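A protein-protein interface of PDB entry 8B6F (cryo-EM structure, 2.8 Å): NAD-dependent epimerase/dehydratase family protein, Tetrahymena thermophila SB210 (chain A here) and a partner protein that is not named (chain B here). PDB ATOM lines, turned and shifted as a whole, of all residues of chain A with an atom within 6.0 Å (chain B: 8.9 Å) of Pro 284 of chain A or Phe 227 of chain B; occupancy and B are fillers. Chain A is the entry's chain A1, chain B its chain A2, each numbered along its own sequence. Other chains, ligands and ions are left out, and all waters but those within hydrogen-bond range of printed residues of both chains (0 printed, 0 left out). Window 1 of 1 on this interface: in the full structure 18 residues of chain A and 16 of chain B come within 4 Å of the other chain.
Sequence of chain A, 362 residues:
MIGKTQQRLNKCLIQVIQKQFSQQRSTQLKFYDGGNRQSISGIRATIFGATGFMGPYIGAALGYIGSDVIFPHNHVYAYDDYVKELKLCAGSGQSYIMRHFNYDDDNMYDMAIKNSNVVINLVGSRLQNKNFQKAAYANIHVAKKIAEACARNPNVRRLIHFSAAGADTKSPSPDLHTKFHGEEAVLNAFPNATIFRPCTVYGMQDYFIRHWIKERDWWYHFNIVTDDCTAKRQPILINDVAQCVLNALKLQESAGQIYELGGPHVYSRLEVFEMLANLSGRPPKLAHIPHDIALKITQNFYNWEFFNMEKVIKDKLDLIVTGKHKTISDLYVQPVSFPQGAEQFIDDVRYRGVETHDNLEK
The side-chain amide oxygen (OD1) of Asn 278 of chain A sits at hydrogen-bond distance from the backbone NH (N) of Phe 227 of chain B (2.8 Å).
OE2 of Glu 274 of chain A lies close to O of Phe 227 of chain B, 3.3 Å away.
The side-chain carboxylate (OD2) of Asp 232 of chain B lies within salt-bridge range of the side-chain amino group (NZ) of Lys 285 of chain A.
O of Leu 286 of chain A lies within hydrogen-bond range of N of Asp 232 of chain B, at 2.9 Å.
The backbone carbonyl oxygen of Glu 274 of chain A lies within hydrogen-bond range of the side-chain amide nitrogen of Asn 278 of chain A (3.0 Å).
Among the printed residues, pairs that only touch across the chains: Asn 278 of chain A with Asn 226 of chain B (3.3 Å), Pro 284 of chain A with Phe 227 of chain B (3.4 Å), Gly 281 of chain A with Phe 227 of chain B (3.7 Å), Leu 286 of chain A with Gln 230 of chain B (3.8 Å) and Glu 274 of chain A with Ala 229 of chain B (3.9 Å).
Pro 284 of chain A touches one residue of chain B.
Phe 227 of chain B touches just these residues of chain A: Glu 274, Asn 278, Gly 281 and Pro 284.
No residue of chain B comes within 4 Å of Pro 283 of chain A.
Of the printed residues of chain A, Gln 230 of chain B touches Leu 286.
Printed residues of chain A within 4 Å of Ala 229 of chain B: Glu 274.
Printed residues of chain B within 4 Å of Lys 285 of chain A: Asp 232 (3.7 Å).
Of the printed residues of chain B, Leu 286 of chain A touches Gln 230 (3.8 Å) and Asp 232 (2.9 Å).
Of the printed residues of chain A, Asn 226 of chain B touches Asn 278 (3.3 Å).
Ala 277 of chain A touches none of the printed residues of chain B.
The nearest residue of chain B that does not touch Pro 284 of chain A is Ala 229 of chain B (4.04 Å).
Printed residues of chain B that touch a printed residue of chain A: Asn 226, Phe 227, Ala 229, Gln 230 and Asp 232.
Hydrophobic or aromatic side chains of chain A within 4 Å of the printed part of chain B: Pro 284 and Leu 286.
Among the printed residues, Asp or Glu carboxylates within 4 Å of a Lys or Arg side-chain nitrogen of the other chain: Lys 285 of chain A with Asp 232 of chain B (3.7 Å).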
ATOM      1  N   ARG A 216      -0.485 -15.263   4.788  1.00  0.00           N
ATOM      2  CA  ARG A 216      -1.252 -14.502   5.766  1.00  0.00           C
ATOM      3  C   ARG A 216      -1.685 -15.372   6.937  1.00  0.00           C
ATOM      4  O   ARG A 216      -1.795 -14.877   8.063  1.00  0.00           O
ATOM      5  CB  ARG A 216      -2.475 -13.860   5.113  1.00  0.00           C
ATOM      6  CG  ARG A 216      -3.337 -13.048   6.081  1.00  0.00           C
ATOM      7  CD  ARG A 216      -2.516 -12.014   6.844  1.00  0.00           C
ATOM      8  NE  ARG A 216      -3.323 -11.222   7.764  1.00  0.00           N
ATOM      9  CZ  ARG A 216      -3.956 -10.102   7.443  1.00  0.00           C
ATOM     10  NH1 ARG A 216      -3.922  -9.614   6.213  1.00  0.00           N
ATOM     11  NH2 ARG A 216      -4.640  -9.452   8.380  1.00  0.00           N
ATOM     12  N   PHE A 273      -3.360  -6.850  -3.773  1.00  0.00           N
ATOM     13  CA  PHE A 273      -3.570  -7.049  -2.343  1.00  0.00           C
ATOM     14  C   PHE A 273      -4.897  -6.448  -1.903  1.00  0.00           C
ATOM     15  O   PHE A 273      -5.652  -7.073  -1.150  1.00  0.00           O
ATOM     16  CB  PHE A 273      -2.418  -6.434  -1.548  1.00  0.00           C
ATOM     17  CG  PHE A 273      -1.170  -7.266  -1.540  1.00  0.00           C
ATOM     18  CD1 PHE A 273      -1.149  -8.502  -0.916  1.00  0.00           C
ATOM     19  CD2 PHE A 273      -0.009  -6.800  -2.131  1.00  0.00           C
ATOM     20  CE1 PHE A 273       0.001  -9.265  -0.899  1.00  0.00           C
ATOM     21  CE2 PHE A 273       1.144  -7.557  -2.118  1.00  0.00           C
ATOM     22  CZ  PHE A 273       1.150  -8.792  -1.501  1.00  0.00           C
ATOM     23  N   GLU A 274      -5.197  -5.234  -2.364  1.00  0.00           N
ATOM     24  CA  GLU A 274      -6.449  -4.587  -1.984  1.00  0.00           C
ATOM     25  C   GLU A 274      -7.652  -5.385  -2.473  1.00  0.00           C
ATOM     26  O   GLU A 274      -8.627  -5.562  -1.733  1.00  0.00           O
ATOM     27  CB  GLU A 274      -6.489  -3.164  -2.543  1.00  0.00           C
ATOM     28  CG  GLU A 274      -7.780  -2.415  -2.252  1.00  0.00           C
ATOM     29  CD  GLU A 274      -7.778  -1.013  -2.826  1.00  0.00           C
ATOM     30  OE1 GLU A 274      -6.727  -0.588  -3.350  1.00  0.00           O
ATOM     31  OE2 GLU A 274      -8.826  -0.337  -2.758  1.00  0.00           O
ATOM     32  N   ALA A 277      -8.016  -8.543  -0.347  1.00  0.00           N
ATOM     33  CA  ALA A 277      -8.511  -8.202   0.981  1.00  0.00           C
ATOM     34  C   ALA A 277      -9.998  -7.880   0.945  1.00  0.00           C
ATOM     35  O   ALA A 277     -10.762  -8.339   1.802  1.00  0.00           O
ATOM     36  CB  ALA A 277      -7.722  -7.023   1.547  1.00  0.00           C
ATOM     37  N   ASN A 278     -10.429  -7.095  -0.043  1.00  0.00           N
ATOM     38  CA  ASN A 278     -11.842  -6.747  -0.142  1.00  0.00           C
ATOM     39  C   ASN A 278     -12.700  -7.974  -0.412  1.00  0.00           C
ATOM     40  O   ASN A 278     -13.772  -8.133   0.181  1.00  0.00           O
ATOM     41  CB  ASN A 278     -12.049  -5.705  -1.241  1.00  0.00           C
ATOM     42  CG  ASN A 278     -11.448  -4.360  -0.890  1.00  0.00           C
ATOM     43  OD1 ASN A 278     -11.438  -3.957   0.271  1.00  0.00           O
ATOM     44  ND2 ASN A 278     -10.942  -3.659  -1.896  1.00  0.00           N
ATOM     45  N   GLY A 281     -12.616 -10.271   2.812  1.00  0.00           N
ATOM     46  CA  GLY A 281     -12.977  -9.644   4.063  1.00  0.00           C
ATOM     47  C   GLY A 281     -11.834  -9.467   5.038  1.00  0.00           C
ATOM     48  O   GLY A 281     -12.025  -8.821   6.076  1.00  0.00           O
ATOM     49  N   ARG A 282     -10.659 -10.013   4.748  1.00  0.00           N
ATOM     50  CA  ARG A 282      -9.526  -9.899   5.657  1.00  0.00           C
ATOM     51  C   ARG A 282      -8.907  -8.510   5.543  1.00  0.00           C
ATOM     52  O   ARG A 282      -8.542  -8.094   4.440  1.00  0.00           O
ATOM     53  CB  ARG A 282      -8.472 -10.954   5.338  1.00  0.00           C
ATOM     54  CG  ARG A 282      -8.899 -12.378   5.635  1.00  0.00           C
ATOM     55  CD  ARG A 282      -7.763 -13.350   5.360  1.00  0.00           C
ATOM     56  NE  ARG A 282      -8.082 -14.705   5.794  1.00  0.00           N
ATOM     57  CZ  ARG A 282      -7.241 -15.728   5.736  1.00  0.00           C
ATOM     58  NH1 ARG A 282      -6.013 -15.589   5.262  1.00  0.00           N
ATOM     59  NH2 ARG A 282      -7.639 -16.921   6.167  1.00  0.00           N
ATOM     60  N   PRO A 283      -8.770  -7.771   6.641  1.00  0.00           N
ATOM     61  CA  PRO A 283      -8.124  -6.460   6.566  1.00  0.00           C
ATOM     62  C   PRO A 283      -6.712  -6.586   6.022  1.00  0.00           C
ATOM     63  O   PRO A 283      -5.999  -7.544   6.355  1.00  0.00           O
ATOM     64  CB  PRO A 283      -8.119  -5.980   8.025  1.00  0.00           C
ATOM     65  CG  PRO A 283      -9.225  -6.718   8.669  1.00  0.00           C
ATOM     66  CD  PRO A 283      -9.264  -8.056   7.999  1.00  0.00           C
ATOM     67  N   PRO A 284      -6.270  -5.652   5.184  1.00  0.00           N
ATOM     68  CA  PRO A 284      -4.915  -5.750   4.635  1.00  0.00           C
ATOM     69  C   PRO A 284      -3.866  -5.234   5.603  1.00  0.00           C
ATOM     70  O   PRO A 284      -4.101  -4.321   6.395  1.00  0.00           O
ATOM     71  CB  PRO A 284      -4.974  -4.875   3.374  1.00  0.00           C
ATOM     72  CG  PRO A 284      -6.335  -4.226   3.368  1.00  0.00           C
ATOM     73  CD  PRO A 284      -6.944  -4.436   4.708  1.00  0.00           C
ATOM     74  N   LYS A 285      -2.689  -5.850   5.531  1.00  0.00           N
ATOM     75  CA  LYS A 285      -1.538  -5.386   6.300  1.00  0.00           C
ATOM     76  C   LYS A 285      -0.288  -5.861   5.576  1.00  0.00           C
ATOM     77  O   LYS A 285      -0.051  -7.068   5.483  1.00  0.00           O
ATOM     78  CB  LYS A 285      -1.586  -5.909   7.730  1.00  0.00           C
ATOM     79  CG  LYS A 285      -0.386  -5.510   8.585  1.00  0.00           C
ATOM     80  CD  LYS A 285      -0.242  -4.004   8.733  1.00  0.00           C
ATOM     81  CE  LYS A 285      -1.402  -3.403   9.509  1.00  0.00           C
ATOM     82  NZ  LYS A 285      -1.204  -1.949   9.761  1.00  0.00           N
ATOM     83  N   LEU A 286       0.502  -4.919   5.072  1.00  0.00           N
ATOM     84  CA  LEU A 286       1.733  -5.218   4.355  1.00  0.00           C
ATOM     85  C   LEU A 286       2.909  -4.760   5.201  1.00  0.00           C
ATOM     86  O   LEU A 286       3.038  -3.566   5.493  1.00  0.00           O
ATOM     87  CB  LEU A 286       1.750  -4.526   2.992  1.00  0.00           C
ATOM     88  CG  LEU A 286       0.546  -4.804   2.092  1.00  0.00           C
ATOM     89  CD1 LEU A 286       0.609  -3.948   0.841  1.00  0.00           C
ATOM     90  CD2 LEU A 286       0.478  -6.277   1.728  1.00  0.00           C
ATOM     91  N   LYS B 224     -20.445  -0.692   5.183  1.00  0.00           N
ATOM     92  CA  LYS B 224     -19.083  -1.192   5.303  1.00  0.00           C
ATOM     93  C   LYS B 224     -18.246  -0.653   4.152  1.00  0.00           C
ATOM     94  O   LYS B 224     -18.651  -0.745   2.989  1.00  0.00           O
ATOM     95  CB  LYS B 224     -19.067  -2.721   5.305  1.00  0.00           C
ATOM     96  CG  LYS B 224     -20.021  -3.339   6.322  1.00  0.00           C
ATOM     97  CD  LYS B 224     -19.867  -4.851   6.403  1.00  0.00           C
ATOM     98  CE  LYS B 224     -20.346  -5.542   5.136  1.00  0.00           C
ATOM     99  NZ  LYS B 224     -21.787  -5.283   4.861  1.00  0.00           N
ATOM    100  N   SER B 225     -17.080  -0.104   4.477  1.00  0.00           N
ATOM    101  CA  SER B 225     -16.196   0.512   3.497  1.00  0.00           C
ATOM    102  C   SER B 225     -15.073  -0.450   3.138  1.00  0.00           C
ATOM    103  O   SER B 225     -14.448  -1.039   4.024  1.00  0.00           O
ATOM    104  CB  SER B 225     -15.617   1.821   4.036  1.00  0.00           C
ATOM    105  OG  SER B 225     -14.950   1.612   5.268  1.00  0.00           O
ATOM    106  N   ASN B 226     -14.819  -0.601   1.841  1.00  0.00           N
ATOM    107  CA  ASN B 226     -13.746  -1.476   1.390  1.00  0.00           C
ATOM    108  C   ASN B 226     -12.399  -0.964   1.881  1.00  0.00           C
ATOM    109  O   ASN B 226     -12.172   0.241   2.006  1.00  0.00           O
ATOM    110  CB  ASN B 226     -13.739  -1.571  -0.136  1.00  0.00           C
ATOM    111  CG  ASN B 226     -14.954  -2.288  -0.681  1.00  0.00           C
ATOM    112  OD1 ASN B 226     -15.950  -2.465   0.019  1.00  0.00           O
ATOM    113  ND2 ASN B 226     -14.879  -2.704  -1.939  1.00  0.00           N
ATOM    114  N   PHE B 227     -11.499  -1.900   2.161  1.00  0.00           N
ATOM    115  CA  PHE B 227     -10.186  -1.547   2.673  1.00  0.00           C
ATOM    116  C   PHE B 227      -9.319  -0.943   1.575  1.00  0.00           C
ATOM    117  O   PHE B 227      -9.473  -1.244   0.389  1.00  0.00           O
ATOM    118  CB  PHE B 227      -9.491  -2.776   3.256  1.00  0.00           C
ATOM    119  CG  PHE B 227     -10.349  -3.573   4.193  1.00  0.00           C
ATOM    120  CD1 PHE B 227     -10.494  -3.191   5.516  1.00  0.00           C
ATOM    121  CD2 PHE B 227     -11.001  -4.714   3.754  1.00  0.00           C
ATOM    122  CE1 PHE B 227     -11.279  -3.927   6.381  1.00  0.00           C
ATOM    123  CE2 PHE B 227     -11.788  -5.452   4.613  1.00  0.00           C
ATOM    124  CZ  PHE B 227     -11.927  -5.057   5.930  1.00  0.00           C
ATOM    125  N   ILE B 228      -8.397  -0.076   1.987  1.00  0.00           N
ATOM    126  CA  ILE B 228      -7.358   0.466   1.118  1.00  0.00           C
ATOM    127  C   ILE B 228      -6.022  -0.061   1.616  1.00  0.00           C
ATOM    128  O   ILE B 228      -5.683   0.104   2.794  1.00  0.00           O
ATOM    129  CB  ILE B 228      -7.371   2.004   1.100  1.00  0.00           C
ATOM    130  CG1 ILE B 228      -8.690   2.516   0.517  1.00  0.00           C
ATOM    131  CG2 ILE B 228      -6.190   2.539   0.294  1.00  0.00           C
ATOM    132  CD1 ILE B 228      -8.874   4.014   0.626  1.00  0.00           C
ATOM    133  N   ALA B 229      -5.268  -0.691   0.722  1.00  0.00           N
ATOM    134  CA  ALA B 229      -4.010  -1.326   1.085  1.00  0.00           C
ATOM    135  C   ALA B 229      -2.856  -0.355   0.879  1.00  0.00           C
ATOM    136  O   ALA B 229      -2.727   0.251  -0.190  1.00  0.00           O
ATOM    137  CB  ALA B 229      -3.789  -2.592   0.257  1.00  0.00           C
ATOM    138  N   GLN B 230      -2.026  -0.207   1.907  1.00  0.00           N
ATOM    139  CA  GLN B 230      -0.821   0.603   1.840  1.00  0.00           C
ATOM    140  C   GLN B 230       0.337  -0.182   2.436  1.00  0.00           C
ATOM    141  O   GLN B 230       0.139  -1.068   3.272  1.00  0.00           O
ATOM    142  CB  GLN B 230      -0.986   1.936   2.586  1.00  0.00           C
ATOM    143  CG  GLN B 230      -1.223   1.788   4.081  1.00  0.00           C
ATOM    144  CD  GLN B 230      -1.222   3.119   4.805  1.00  0.00           C
ATOM    145  OE1 GLN B 230      -1.292   4.176   4.183  1.00  0.00           O
ATOM    146  NE2 GLN B 230      -1.138   3.071   6.128  1.00  0.00           N
ATOM    147  N   VAL B 231       1.544   0.148   1.998  1.00  0.00           N
ATOM    148  CA  VAL B 231       2.743  -0.517   2.494  1.00  0.00           C
ATOM    149  C   VAL B 231       3.139   0.108   3.824  1.00  0.00           C
ATOM    150  O   VAL B 231       3.215   1.335   3.948  1.00  0.00           O
ATOM    151  CB  VAL B 231       3.884  -0.418   1.469  1.00  0.00           C
ATOM    152  CG1 VAL B 231       5.100  -1.191   1.951  1.00  0.00           C
ATOM    153  CG2 VAL B 231       3.426  -0.930   0.114  1.00  0.00           C
ATOM    154  N   ASP B 232       3.380  -0.736   4.823  1.00  0.00           N
ATOM    155  CA  ASP B 232       3.778  -0.295   6.156  1.00  0.00           C
ATOM    156  C   ASP B 232       5.296  -0.390   6.252  1.00  0.00           C
ATOM    157  O   ASP B 232       5.856  -1.491   6.265  1.00  0.00           O
ATOM    158  CB  ASP B 232       3.103  -1.145   7.229  1.00  0.00           C
ATOM    159  CG  ASP B 232       3.247  -0.557   8.617  1.00  0.00           C
ATOM    160  OD1 ASP B 232       4.277   0.092   8.887  1.00  0.00           O
ATOM    161  OD2 ASP B 232       2.327  -0.743   9.439  1.00  0.00           O
